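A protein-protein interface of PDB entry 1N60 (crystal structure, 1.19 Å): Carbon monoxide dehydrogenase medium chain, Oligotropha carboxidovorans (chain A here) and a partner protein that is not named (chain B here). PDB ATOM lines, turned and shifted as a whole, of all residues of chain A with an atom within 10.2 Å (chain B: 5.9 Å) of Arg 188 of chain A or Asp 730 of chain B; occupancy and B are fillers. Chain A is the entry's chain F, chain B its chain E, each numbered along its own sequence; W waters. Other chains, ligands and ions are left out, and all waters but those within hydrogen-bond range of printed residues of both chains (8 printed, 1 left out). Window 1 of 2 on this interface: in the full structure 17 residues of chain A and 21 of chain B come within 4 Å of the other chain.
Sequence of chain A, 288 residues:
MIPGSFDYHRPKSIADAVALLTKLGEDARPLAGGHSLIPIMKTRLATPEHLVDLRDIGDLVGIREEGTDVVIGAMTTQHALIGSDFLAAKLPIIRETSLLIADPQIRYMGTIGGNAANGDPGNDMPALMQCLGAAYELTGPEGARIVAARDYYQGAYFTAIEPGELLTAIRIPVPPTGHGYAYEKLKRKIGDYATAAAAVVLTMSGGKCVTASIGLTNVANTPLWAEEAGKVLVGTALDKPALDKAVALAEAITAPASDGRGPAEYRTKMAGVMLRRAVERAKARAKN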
ATOM      1  N   LEU A 100      27.548 -19.062  21.764  1.00  0.00           N
ATOM      2  CA  LEU A 100      27.094 -18.295  20.634  1.00  0.00           C
ATOM      3  C   LEU A 100      27.857 -16.991  20.449  1.00  0.00           C
ATOM      4  O   LEU A 100      27.578 -16.230  19.557  1.00  0.00           O
ATOM      5  CB  LEU A 100      25.600 -18.003  20.752  1.00  0.00           C
ATOM      6  CG  LEU A 100      24.793 -19.282  20.630  1.00  0.00           C
ATOM      7  CD1 LEU A 100      23.397 -19.036  21.108  1.00  0.00           C
ATOM      8  CD2 LEU A 100      24.756 -19.823  19.249  1.00  0.00           C
ATOM      9  N   GLY A 122      26.110  -4.970  20.064  1.00  0.00           N
ATOM     10  CA  GLY A 122      26.306  -6.247  19.530  1.00  0.00           C
ATOM     11  C   GLY A 122      26.587  -7.278  20.587  1.00  0.00           C
ATOM     12  O   GLY A 122      26.354  -8.455  20.369  1.00  0.00           O
ATOM     13  N   LYS A 185      19.904 -16.958  18.825  1.00  0.00           N
ATOM     14  CA  LYS A 185      20.619 -15.916  18.141  1.00  0.00           C
ATOM     15  C   LYS A 185      20.553 -16.148  16.640  1.00  0.00           C
ATOM     16  O   LYS A 185      20.790 -17.272  16.182  1.00  0.00           O
ATOM     17  CB  LYS A 185      22.067 -15.915  18.577  1.00  0.00           C
ATOM     18  CG  LYS A 185      22.971 -14.887  17.909  1.00  0.00           C
ATOM     19  CD  LYS A 185      24.289 -14.790  18.619  1.00  0.00           C
ATOM     20  CE  LYS A 185      25.244 -13.855  17.977  1.00  0.00           C
ATOM     21  NZ  LYS A 185      26.539 -13.749  18.738  1.00  0.00           N
ATOM     22  N   LEU A 186      20.301 -15.128  15.876  1.00  0.00           N
ATOM     23  CA  LEU A 186      20.327 -15.130  14.422  1.00  0.00           C
ATOM     24  C   LEU A 186      21.536 -14.338  14.031  1.00  0.00           C
ATOM     25  O   LEU A 186      21.687 -13.214  14.465  1.00  0.00           O
ATOM     26  CB  LEU A 186      19.061 -14.511  13.897  1.00  0.00           C
ATOM     27  CG  LEU A 186      18.977 -14.441  12.399  1.00  0.00           C
ATOM     28  CD1 LEU A 186      18.938 -15.801  11.734  1.00  0.00           C
ATOM     29  CD2 LEU A 186      17.754 -13.653  11.982  1.00  0.00           C
ATOM     30  N   LYS A 187      22.407 -14.950  13.236  1.00  0.00           N
ATOM     31  CA  LYS A 187      23.633 -14.278  12.837  1.00  0.00           C
ATOM     32  C   LYS A 187      24.022 -14.697  11.456  1.00  0.00           C
ATOM     33  O   LYS A 187      23.583 -15.702  10.982  1.00  0.00           O
ATOM     34  CB  LYS A 187      24.752 -14.535  13.817  1.00  0.00           C
ATOM     35  CG  LYS A 187      25.098 -16.015  13.913  1.00  0.00           C
ATOM     36  CD  LYS A 187      25.909 -16.362  15.109  1.00  0.00           C
ATOM     37  CE  LYS A 187      26.505 -17.709  15.073  1.00  0.00           C
ATOM     38  NZ  LYS A 187      25.574 -18.789  15.062  1.00  0.00           N
ATOM     39  N   ARG A 188      24.887 -13.917  10.841  1.00  0.00           N
ATOM     40  CA  ARG A 188      25.292 -14.258   9.483  1.00  0.00           C
ATOM     41  C   ARG A 188      26.268 -15.402   9.405  1.00  0.00           C
ATOM     42  O   ARG A 188      26.316 -16.080   8.384  1.00  0.00           O
ATOM     43  CB  ARG A 188      25.906 -13.045   8.802  1.00  0.00           C
ATOM     44  CG  ARG A 188      24.924 -11.975   8.478  1.00  0.00           C
ATOM     45  CD  ARG A 188      25.509 -10.670   7.976  1.00  0.00           C
ATOM     46  NE  ARG A 188      26.343 -10.067   9.004  1.00  0.00           N
ATOM     47  CZ  ARG A 188      27.002  -8.961   8.846  1.00  0.00           C
ATOM     48  NH1 ARG A 188      26.967  -8.302   7.679  1.00  0.00           N
ATOM     49  NH2 ARG A 188      27.704  -8.468   9.846  1.00  0.00           N
ATOM     50  N   LYS A 189      27.067 -15.622  10.430  1.00  0.00           N
ATOM     51  CA  LYS A 189      28.051 -16.659  10.473  1.00  0.00           C
ATOM     52  C   LYS A 189      28.565 -16.642  11.897  1.00  0.00           C
ATOM     53  O   LYS A 189      28.350 -15.749  12.673  1.00  0.00           O
ATOM     54  CB  LYS A 189      29.221 -16.462   9.467  1.00  0.00           C
ATOM     55  CG  LYS A 189      29.764 -15.024   9.488  1.00  0.00           C
ATOM     56  CD  LYS A 189      31.005 -14.832   8.640  1.00  0.00           C
ATOM     57  CE  LYS A 189      32.222 -15.258   9.377  1.00  0.00           C
ATOM     58  NZ  LYS A 189      33.449 -15.011   8.542  1.00  0.00           N
ATOM     59  N   ILE A 190      29.335 -17.675  12.192  1.00  0.00           N
ATOM     60  CA  ILE A 190      30.163 -17.749  13.378  1.00  0.00           C
ATOM     61  C   ILE A 190      30.913 -16.467  13.551  1.00  0.00           C
ATOM     62  O   ILE A 190      31.559 -15.957  12.666  1.00  0.00           O
ATOM     63  CB  ILE A 190      31.247 -18.932  13.272  1.00  0.00           C
ATOM     64  CG1 ILE A 190      30.580 -20.249  13.312  1.00  0.00           C
ATOM     65  CG2 ILE A 190      32.285 -18.790  14.365  1.00  0.00           C
ATOM     66  CD1 ILE A 190      29.695 -20.528  14.540  1.00  0.00           C
ATOM     67  N   GLY A 191      30.798 -15.957  14.788  1.00  0.00           N
ATOM     68  CA  GLY A 191      31.549 -14.810  15.209  1.00  0.00           C
ATOM     69  C   GLY A 191      30.786 -13.525  15.023  1.00  0.00           C
ATOM     70  O   GLY A 191      31.174 -12.522  15.531  1.00  0.00           O
ATOM     71  N   ASP A 192      29.714 -13.527  14.248  1.00  0.00           N
ATOM     72  CA  ASP A 192      29.004 -12.294  13.949  1.00  0.00           C
ATOM     73  C   ASP A 192      28.088 -11.893  15.091  1.00  0.00           C
ATOM     74  O   ASP A 192      27.461 -12.718  15.764  1.00  0.00           O
ATOM     75  CB  ASP A 192      28.161 -12.507  12.702  1.00  0.00           C
ATOM     76  CG  ASP A 192      27.537 -11.293  12.081  1.00  0.00           C
ATOM     77  OD1 ASP A 192      28.044 -10.180  12.302  1.00  0.00           O
ATOM     78  OD2 ASP A 192      26.411 -11.438  11.448  1.00  0.00           O
ATOM     79  N   TYR A 193      28.032 -10.606  15.349  1.00  0.00           N
ATOM     80  CA  TYR A 193      27.048 -10.058  16.275  1.00  0.00           C
ATOM     81  C   TYR A 193      25.671 -10.328  15.703  1.00  0.00           C
ATOM     82  O   TYR A 193      25.461 -10.368  14.493  1.00  0.00           O
ATOM     83  CB  TYR A 193      27.281  -8.576  16.465  1.00  0.00           C
ATOM     84  CG  TYR A 193      28.646  -8.287  16.992  1.00  0.00           C
ATOM     85  CD1 TYR A 193      28.950  -8.483  18.324  1.00  0.00           C
ATOM     86  CD2 TYR A 193      29.672  -7.900  16.143  1.00  0.00           C
ATOM     87  CE1 TYR A 193      30.192  -8.214  18.798  1.00  0.00           C
ATOM     88  CE2 TYR A 193      30.945  -7.668  16.621  1.00  0.00           C
ATOM     89  CZ  TYR A 193      31.191  -7.857  17.942  1.00  0.00           C
ATOM     90  OH  TYR A 193      32.427  -7.605  18.439  1.00  0.00           O
ATOM     91  N   ALA A 194      24.693 -10.428  16.589  1.00  0.00           N
ATOM     92  CA  ALA A 194      23.354 -10.880  16.172  1.00  0.00           C
ATOM     93  C   ALA A 194      22.708  -9.927  15.243  1.00  0.00           C
ATOM     94  O   ALA A 194      22.651  -8.703  15.472  1.00  0.00           O
ATOM     95  CB  ALA A 194      22.482 -11.070  17.373  1.00  0.00           C
ATOM     96  N   THR A 195      22.079 -10.495  14.241  1.00  0.00           N
ATOM     97  CA  THR A 195      21.018  -9.787  13.563  1.00  0.00           C
ATOM     98  C   THR A 195      19.896  -9.443  14.555  1.00  0.00           C
ATOM     99  O   THR A 195      19.365  -8.331  14.562  1.00  0.00           O
ATOM    100  CB  THR A 195      20.530 -10.719  12.488  1.00  0.00           C
ATOM    101  OG1 THR A 195      21.608 -10.920  11.548  1.00  0.00           O
ATOM    102  CG2 THR A 195      19.383 -10.087  11.726  1.00  0.00           C
ATOM    103  N   ALA A 196      19.579 -10.459  15.368  1.00  0.00           N
ATOM    104  CA  ALA A 196      18.717 -10.293  16.543  1.00  0.00           C
ATOM    105  C   ALA A 196      18.929 -11.502  17.419  1.00  0.00           C
ATOM    106  O   ALA A 196      19.247 -12.606  16.907  1.00  0.00           O
ATOM    107  CB  ALA A 196      17.269 -10.230  16.120  1.00  0.00           C
ATOM    108  N   ASN A 218      20.933  -6.643  20.340  1.00  0.00           N
ATOM    109  CA  ASN A 218      21.360  -5.985  19.108  1.00  0.00           C
ATOM    110  C   ASN A 218      20.226  -5.563  18.219  1.00  0.00           C
ATOM    111  O   ASN A 218      20.377  -5.531  17.017  1.00  0.00           O
ATOM    112  CB  ASN A 218      22.416  -6.828  18.366  1.00  0.00           C
ATOM    113  CG  ASN A 218      23.363  -5.977  17.581  1.00  0.00           C
ATOM    114  OD1 ASN A 218      23.605  -4.812  17.904  1.00  0.00           O
ATOM    115  ND2 ASN A 218      24.013  -6.588  16.610  1.00  0.00           N
ATOM    116  N   SER A 258      20.078  -0.341  10.650  1.00  0.00           N
ATOM    117  CA  SER A 258      20.050  -0.921   9.289  1.00  0.00           C
ATOM    118  C   SER A 258      21.488  -1.048   8.846  1.00  0.00           C
ATOM    119  O   SER A 258      22.183  -0.056   8.710  1.00  0.00           O
ATOM    120  CB  SER A 258      19.281  -0.022   8.340  1.00  0.00           C
ATOM    121  OG  SER A 258      17.879  -0.031   8.694  1.00  0.00           O
ATOM    122  N   ASP A 259      21.985  -2.275   8.718  1.00  0.00           N
ATOM    123  CA  ASP A 259      23.351  -2.484   8.369  1.00  0.00           C
ATOM    124  C   ASP A 259      23.476  -3.738   7.534  1.00  0.00           C
ATOM    125  O   ASP A 259      22.514  -4.150   6.893  1.00  0.00           O
ATOM    126  CB  ASP A 259      24.248  -2.401   9.638  1.00  0.00           C
ATOM    127  CG  ASP A 259      24.049  -3.485  10.636  1.00  0.00           C
ATOM    128  OD1 ASP A 259      23.663  -4.619  10.281  1.00  0.00           O
ATOM    129  OD2 ASP A 259      24.286  -3.288  11.855  1.00  0.00           O
ATOM    130  N   GLY A 260      24.652  -4.316   7.450  1.00  0.00           N
ATOM    131  CA  GLY A 260      24.879  -5.493   6.638  1.00  0.00           C
ATOM    132  C   GLY A 260      24.037  -6.662   7.076  1.00  0.00           C
ATOM    133  O   GLY A 260      23.841  -7.581   6.302  1.00  0.00           O
ATOM    134  N   ARG A 261      23.499  -6.664   8.288  1.00  0.00           N
ATOM    135  CA  ARG A 261      22.650  -7.718   8.737  1.00  0.00           C
ATOM    136  C   ARG A 261      21.217  -7.563   8.273  1.00  0.00           C
ATOM    137  O   ARG A 261      20.386  -8.462   8.442  1.00  0.00           O
ATOM    138  CB  ARG A 261      22.683  -7.755  10.260  1.00  0.00           C
ATOM    139  CG  ARG A 261      24.038  -8.074  10.786  1.00  0.00           C
ATOM    140  CD  ARG A 261      24.184  -7.851  12.296  1.00  0.00           C
ATOM    141  NE  ARG A 261      25.554  -7.988  12.729  1.00  0.00           N
ATOM    142  CZ  ARG A 261      26.466  -7.056  12.583  1.00  0.00           C
ATOM    143  NH1 ARG A 261      26.175  -5.887  12.082  1.00  0.00           N
ATOM    144  NH2 ARG A 261      27.687  -7.319  12.881  1.00  0.00           N
ATOM    145  N   GLY A 262      20.936  -6.449   7.636  1.00  0.00           N
ATOM    146  CA  GLY A 262      19.605  -6.216   7.125  1.00  0.00           C
ATOM    147  C   GLY A 262      19.028  -4.924   7.686  1.00  0.00           C
ATOM    148  O   GLY A 262      19.590  -4.292   8.566  1.00  0.00           O
ATOM    149  N   PRO A 263      17.911  -4.544   7.110  1.00  0.00           N
ATOM    150  CA  PRO A 263      17.266  -3.289   7.501  1.00  0.00           C
ATOM    151  C   PRO A 263      16.527  -3.436   8.779  1.00  0.00           C
ATOM    152  O   PRO A 263      16.191  -4.552   9.210  1.00  0.00           O
ATOM    153  CB  PRO A 263      16.298  -3.027   6.369  1.00  0.00           C
ATOM    154  CG  PRO A 263      15.932  -4.415   5.893  1.00  0.00           C
ATOM    155  CD  PRO A 263      17.200  -5.241   6.033  1.00  0.00           C
ATOM    156  N   TYR A 266      13.458  -5.789   9.193  1.00  0.00           N
ATOM    157  CA  TYR A 266      13.751  -7.205   9.246  1.00  0.00           C
ATOM    158  C   TYR A 266      14.198  -7.568  10.644  1.00  0.00           C
ATOM    159  O   TYR A 266      13.795  -8.580  11.220  1.00  0.00           O
ATOM    160  CB  TYR A 266      14.893  -7.532   8.249  1.00  0.00           C
ATOM    161  CG  TYR A 266      15.467  -8.892   8.375  1.00  0.00           C
ATOM    162  CD1 TYR A 266      14.666  -9.979   8.237  1.00  0.00           C
ATOM    163  CD2 TYR A 266      16.829  -9.111   8.638  1.00  0.00           C
ATOM    164  CE1 TYR A 266      15.175 -11.272   8.287  1.00  0.00           C
ATOM    165  CE2 TYR A 266      17.300 -10.392   8.719  1.00  0.00           C
ATOM    166  CZ  TYR A 266      16.503 -11.475   8.548  1.00  0.00           C
ATOM    167  OH  TYR A 266      17.047 -12.739   8.627  1.00  0.00           O
ATOM    168  N   ARG A 267      15.106  -6.764  11.160  1.00  0.00           N
ATOM    169  CA  ARG A 267      15.663  -7.078  12.449  1.00  0.00           C
ATOM    170  C   ARG A 267      14.622  -7.026  13.581  1.00  0.00           C
ATOM    171  O   ARG A 267      14.655  -7.840  14.509  1.00  0.00           O
ATOM    172  CB  ARG A 267      16.821  -6.143  12.718  1.00  0.00           C
ATOM    173  CG  ARG A 267      17.944  -6.387  11.691  1.00  0.00           C
ATOM    174  CD  ARG A 267      19.131  -5.499  11.946  1.00  0.00           C
ATOM    175  NE  ARG A 267      19.898  -5.975  13.054  1.00  0.00           N
ATOM    176  CZ  ARG A 267      21.055  -5.446  13.341  1.00  0.00           C
ATOM    177  NH1 ARG A 267      21.476  -4.361  12.734  1.00  0.00           N
ATOM    178  NH2 ARG A 267      21.803  -6.000  14.263  1.00  0.00           N
ATOM    179  N   MET A 270      12.885 -10.202  13.309  1.00  0.00           N
ATOM    180  CA  MET A 270      13.729 -11.282  13.783  1.00  0.00           C
ATOM    181  C   MET A 270      13.848 -11.283  15.286  1.00  0.00           C
ATOM    182  O   MET A 270      13.951 -12.366  15.867  1.00  0.00           O
ATOM    183  CB  MET A 270      15.114 -11.242  13.152  1.00  0.00           C
ATOM    184  CG  MET A 270      15.091 -11.528  11.655  1.00  0.00           C
ATOM    185  SD  MET A 270      14.271 -13.057  11.197  1.00  0.00           S
ATOM    186  CE  MET A 270      12.603 -12.460  10.735  1.00  0.00           C
ATOM    187  N   MET A 274      13.128 -14.761  17.057  1.00  0.00           N
ATOM    188  CA  MET A 274      14.037 -15.321  18.033  1.00  0.00           C
ATOM    189  C   MET A 274      13.318 -15.476  19.367  1.00  0.00           C
ATOM    190  O   MET A 274      13.518 -16.456  20.084  1.00  0.00           O
ATOM    191  CB  MET A 274      15.265 -14.434  18.143  1.00  0.00           C
ATOM    192  CG  MET A 274      16.156 -14.469  16.911  1.00  0.00           C
ATOM    193  SD  MET A 274      16.701 -16.093  16.377  1.00  0.00           S
ATOM    194  CE  MET A 274      15.639 -16.409  15.133  1.00  0.00           C
ATOM    195  N   GLY B 712      26.051 -14.800   0.322  1.00  0.00           N
ATOM    196  CA  GLY B 712      26.333 -13.696   1.221  1.00  0.00           C
ATOM    197  C   GLY B 712      27.305 -12.625   0.855  1.00  0.00           C
ATOM    198  O   GLY B 712      27.196 -11.539   1.362  1.00  0.00           O
ATOM    199  N   GLU B 714      29.490  -9.655  -0.695  1.00  0.00           N
ATOM    200  CA  GLU B 714      29.252  -8.462  -1.456  1.00  0.00           C
ATOM    201  C   GLU B 714      30.229  -7.390  -1.034  1.00  0.00           C
ATOM    202  O   GLU B 714      30.663  -7.319   0.117  1.00  0.00           O
ATOM    203  CB  GLU B 714      27.828  -7.919  -1.225  1.00  0.00           C
ATOM    204  CG  GLU B 714      27.525  -7.665   0.229  1.00  0.00           C
ATOM    205  CD  GLU B 714      26.075  -7.303   0.510  1.00  0.00           C
ATOM    206  OE1 GLU B 714      25.322  -7.098  -0.457  1.00  0.00           O
ATOM    207  OE2 GLU B 714      25.735  -7.110   1.674  1.00  0.00           O
ATOM    208  N   ARG B 716      29.665  -3.246  -1.472  1.00  0.00           N
ATOM    209  CA  ARG B 716      28.679  -2.296  -1.950  1.00  0.00           C
ATOM    210  C   ARG B 716      29.207  -0.888  -1.791  1.00  0.00           C
ATOM    211  O   ARG B 716      30.206  -0.633  -1.108  1.00  0.00           O
ATOM    212  CB  ARG B 716      27.404  -2.416  -1.142  1.00  0.00           C
ATOM    213  CG  ARG B 716      26.614  -3.658  -1.404  1.00  0.00           C
ATOM    214  CD  ARG B 716      25.451  -3.742  -0.325  1.00  0.00           C
ATOM    215  NE  ARG B 716      25.992  -4.302   0.891  1.00  0.00           N
ATOM    216  CZ  ARG B 716      26.063  -3.845   2.147  1.00  0.00           C
ATOM    217  NH1 ARG B 716      26.688  -4.637   3.009  1.00  0.00           N
ATOM    218  NH2 ARG B 716      25.524  -2.711   2.594  1.00  0.00           N
ATOM    219  N   GLY B 725      30.915  -2.747   3.674  1.00  0.00           N
ATOM    220  CA  GLY B 725      31.082  -4.145   3.888  1.00  0.00           C
ATOM    221  C   GLY B 725      32.440  -4.703   3.559  1.00  0.00           C
ATOM    222  O   GLY B 725      32.607  -5.915   3.571  1.00  0.00           O
ATOM    223  N   ALA B 726      33.419  -3.828   3.388  1.00  0.00           N
ATOM    224  CA  ALA B 726      34.753  -4.200   2.920  1.00  0.00           C
ATOM    225  C   ALA B 726      35.700  -4.497   4.080  1.00  0.00           C
ATOM    226  O   ALA B 726      36.746  -3.881   4.244  1.00  0.00           O
ATOM    227  CB  ALA B 726      35.281  -3.169   1.977  1.00  0.00           C
ATOM    228  N   SER B 727      35.251  -5.395   4.967  1.00  0.00           N
ATOM    229  CA  SER B 727      36.076  -5.950   6.020  1.00  0.00           C
ATOM    230  C   SER B 727      35.451  -7.276   6.395  1.00  0.00           C
ATOM    231  O   SER B 727      34.309  -7.554   6.077  1.00  0.00           O
ATOM    232  CB  SER B 727      36.102  -5.059   7.235  1.00  0.00           C
ATOM    233  OG  SER B 727      35.015  -5.257   8.100  1.00  0.00           O
ATOM    234  N   PHE B 728      36.161  -8.079   7.149  1.00  0.00           N
ATOM    235  CA  PHE B 728      35.642  -9.341   7.554  1.00  0.00           C
ATOM    236  C   PHE B 728      34.554  -9.202   8.650  1.00  0.00           C
ATOM    237  O   PHE B 728      33.965 -10.189   9.039  1.00  0.00           O
ATOM    238  CB  PHE B 728      36.751 -10.295   7.986  1.00  0.00           C
ATOM    239  CG  PHE B 728      37.630 -10.796   6.861  1.00  0.00           C
ATOM    240  CD1 PHE B 728      37.319 -10.589   5.560  1.00  0.00           C
ATOM    241  CD2 PHE B 728      38.795 -11.456   7.146  1.00  0.00           C
ATOM    242  CE1 PHE B 728      38.116 -11.067   4.554  1.00  0.00           C
ATOM    243  CE2 PHE B 728      39.574 -11.988   6.171  1.00  0.00           C
ATOM    244  CZ  PHE B 728      39.264 -11.754   4.883  1.00  0.00           C
ATOM    245  N   MET B 729      34.256  -7.987   9.086  1.00  0.00           N
ATOM    246  CA  MET B 729      33.071  -7.786   9.898  1.00  0.00           C
ATOM    247  C   MET B 729      31.808  -8.134   9.145  1.00  0.00           C
ATOM    248  O   MET B 729      30.797  -8.539   9.732  1.00  0.00           O
ATOM    249  CB  MET B 729      33.005  -6.346  10.402  1.00  0.00           C
ATOM    250  CG  MET B 729      32.083  -6.196  11.635  1.00  0.00           C
ATOM    251  SD  MET B 729      32.808  -6.898  13.105  1.00  0.00           S
ATOM    252  CE  MET B 729      34.135  -6.396  12.946  1.00  0.00           C
ATOM    253  N   ASP B 730      31.821  -7.934   7.836  1.00  0.00           N
ATOM    254  CA  ASP B 730      30.643  -8.053   7.014  1.00  0.00           C
ATOM    255  C   ASP B 730      30.830  -8.945   5.801  1.00  0.00           C
ATOM    256  O   ASP B 730      29.865  -9.539   5.365  1.00  0.00           O
ATOM    257  CB  ASP B 730      30.190  -6.687   6.522  1.00  0.00           C
ATOM    258  CG  ASP B 730      29.743  -5.826   7.647  1.00  0.00           C
ATOM    259  OD1 ASP B 730      28.669  -6.114   8.213  1.00  0.00           O
ATOM    260  OD2 ASP B 730      30.458  -4.912   8.038  1.00  0.00           O
ATOM    261  N   PHE B 731      32.027  -8.991   5.237  1.00  0.00           N
ATOM    262  CA  PHE B 731      32.295  -9.752   4.045  1.00  0.00           C
ATOM    263  C   PHE B 731      32.231 -11.215   4.352  1.00  0.00           C
ATOM    264  O   PHE B 731      33.028 -11.719   5.106  1.00  0.00           O
ATOM    265  CB  PHE B 731      33.638  -9.343   3.476  1.00  0.00           C
ATOM    266  CG  PHE B 731      33.946  -9.924   2.157  1.00  0.00           C
ATOM    267  CD1 PHE B 731      33.446  -9.340   1.021  1.00  0.00           C
ATOM    268  CD2 PHE B 731      34.803 -11.000   2.053  1.00  0.00           C
ATOM    269  CE1 PHE B 731      33.737  -9.880  -0.184  1.00  0.00           C
ATOM    270  CE2 PHE B 731      35.108 -11.521   0.823  1.00  0.00           C
ATOM    271  CZ  PHE B 731      34.618 -10.955  -0.279  1.00  0.00           C
ATOM    272  N   PHE B 732      31.277 -11.890   3.760  1.00  0.00           N
ATOM    273  CA  PHE B 732      30.946 -13.251   4.140  1.00  0.00           C
ATOM    274  C   PHE B 732      31.985 -14.236   3.629  1.00  0.00           C
ATOM    275  O   PHE B 732      32.025 -14.592   2.485  1.00  0.00           O
ATOM    276  CB  PHE B 732      29.584 -13.641   3.541  1.00  0.00           C
ATOM    277  CG  PHE B 732      29.136 -15.006   3.927  1.00  0.00           C
ATOM    278  CD1 PHE B 732      28.842 -15.341   5.231  1.00  0.00           C
ATOM    279  CD2 PHE B 732      28.954 -15.967   2.956  1.00  0.00           C
ATOM    280  CE1 PHE B 732      28.347 -16.601   5.536  1.00  0.00           C
ATOM    281  CE2 PHE B 732      28.523 -17.252   3.278  1.00  0.00           C
ATOM    282  CZ  PHE B 732      28.220 -17.549   4.604  1.00  0.00           C
ATOM    283  N   GLU B 738      29.677 -23.046   8.487  1.00  0.00           N
ATOM    284  CA  GLU B 738      28.706 -22.689   7.437  1.00  0.00           C
ATOM    285  C   GLU B 738      28.968 -23.458   6.148  1.00  0.00           C
ATOM    286  O   GLU B 738      28.112 -23.580   5.345  1.00  0.00           O
ATOM    287  CB  GLU B 738      28.771 -21.207   7.053  1.00  0.00           C
ATOM    288  CG  GLU B 738      28.359 -20.263   8.163  1.00  0.00           C
ATOM    289  CD  GLU B 738      29.381 -20.066   9.259  1.00  0.00           C
ATOM    290  OE1 GLU B 738      30.591 -20.070   8.903  1.00  0.00           O
ATOM    291  OE2 GLU B 738      28.998 -19.801  10.412  1.00  0.00           O
ATOM    292  N   ASP B 794      21.270 -14.010   1.098  1.00  0.00           N
ATOM    293  CA  ASP B 794      21.437 -14.018   2.517  1.00  0.00           C
ATOM    294  C   ASP B 794      20.071 -13.878   3.153  1.00  0.00           C
ATOM    295  O   ASP B 794      19.054 -13.707   2.516  1.00  0.00           O
ATOM    296  CB  ASP B 794      22.455 -12.997   2.974  1.00  0.00           C
ATOM    297  CG  ASP B 794      22.109 -11.565   2.722  1.00  0.00           C
ATOM    298  OD1 ASP B 794      21.057 -11.318   2.100  1.00  0.00           O
ATOM    299  OD2 ASP B 794      22.936 -10.713   3.111  1.00  0.00           O
HETATM  300  O   HOH W   1      34.130  -8.150  16.064  1.00  0.00           O
HETATM  301  O   HOH W   2      23.830  -6.868   3.613  1.00  0.00           O
HETATM  302  O   HOH W   3      26.510  -8.914   5.003  1.00  0.00           O
HETATM  303  O   HOH W   4      33.927 -12.514   7.476  1.00  0.00           O
HETATM  304  O   HOH W   5      30.515  -8.882  12.484  1.00  0.00           O
HETATM  305  O   HOH W   6      23.233 -10.225   5.760  1.00  0.00           O
HETATM  306  O   HOH W   7      27.183  -3.924   8.650  1.00  0.00           O
HETATM  307  O   HOH W   8      29.541 -11.440   9.257  1.00  0.00           O
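OD1 of Asp 730 of chain B lies within salt-bridge range of NH1 of Arg 188 of chain A (2.8 Å). The side-chain carboxylate (OE2) of Glu 738 of chain B is in hydrogen-bond range of the backbone NH (N) of Ile 190 of chain A, 2.8 Å away. O of Met 729 of chain B is in hydrogen-bond range of NH2 of Arg 188 of chain A (3.1 Å).
The side-chain hydroxyl (OG) of Ser 727 of chain B sits at hydrogen-bond distance from the backbone NH (N) of Met 729 of chain B, 3.0 Å away. NH1 of Arg 188 of chain A sits close to O of Gly 260 of chain A (3.5 Å). NE of Arg 188 of chain A is in salt-bridge range of OD2 of Asp 192 of chain A, at 2.8 Å.
Among the printed residues, merely in contact across the chains: Lys 189 of chain A with Glu 738 of chain B and Arg 188 of chain A with Phe 732 of chain B.
Of the printed residues of chain B, Arg 188 of chain A touches Met 729 (3.1 Å), Asp 730 (2.8 Å) and Phe 732 (3.5 Å). Of the printed residues of chain B, Lys 189 of chain A touches Glu 738. Ala 194 of chain A touches none of the printed residues of chain B. No residue of chain A comes within 4 Å of Gly 725 of chain B. No residue of chain A comes within 4 Å of Ser 727 of chain B. Asp 730 of chain B touches one residue of chain A. Printed residues of chain A within 4 Å of Phe 732 of chain B: Arg 188 (3.5 Å). Of the printed residues of chain A, Glu 738 of chain B touches Lys 189 (3.3 Å) and Ile 190 (2.8 Å). The nearest printed residue of chain B that does not touch Arg 188 of chain A is Glu 738 of chain B (4.7 Å).
Hydrophobic or aromatic side chains of chain B within 4 Å of the printed part of chain A: Phe 732. Among the printed residues, 5 pairs touch across the chains. Among the printed residues, Asp or Glu carboxylates within 4 Å of a Lys or Arg side-chain nitrogen of the other chain: Arg 188 of chain A with Asp 730 of chain B.
Water W7 lies within hydrogen-bond range of OD1 of Asp 730 of chain B (2.7 Å) and N of Gly 260 of chain A (2.8 Å). Water W6 bridges OD2 of Asp 794 of chain B (2.7 Å) and O of Gly 260 of chain A (2.8 Å). Water W2 lies within hydrogen-bond range of the side-chain carboxylate (OE2) of Glu 714 of chain B (2.7 Å) and the backbone carbonyl oxygen (O) of Gly 260 of chain A (2.8 Å). Water W1 lies within hydrogen-bond range of OH of Tyr 193 of chain A (3.0 Å) and SD of Met 729 of chain B (3.5 Å). Water W8 bridges O of Met 729 of chain B (3.2 Å) and NE of Arg 188 of chain A (3.5 Å).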
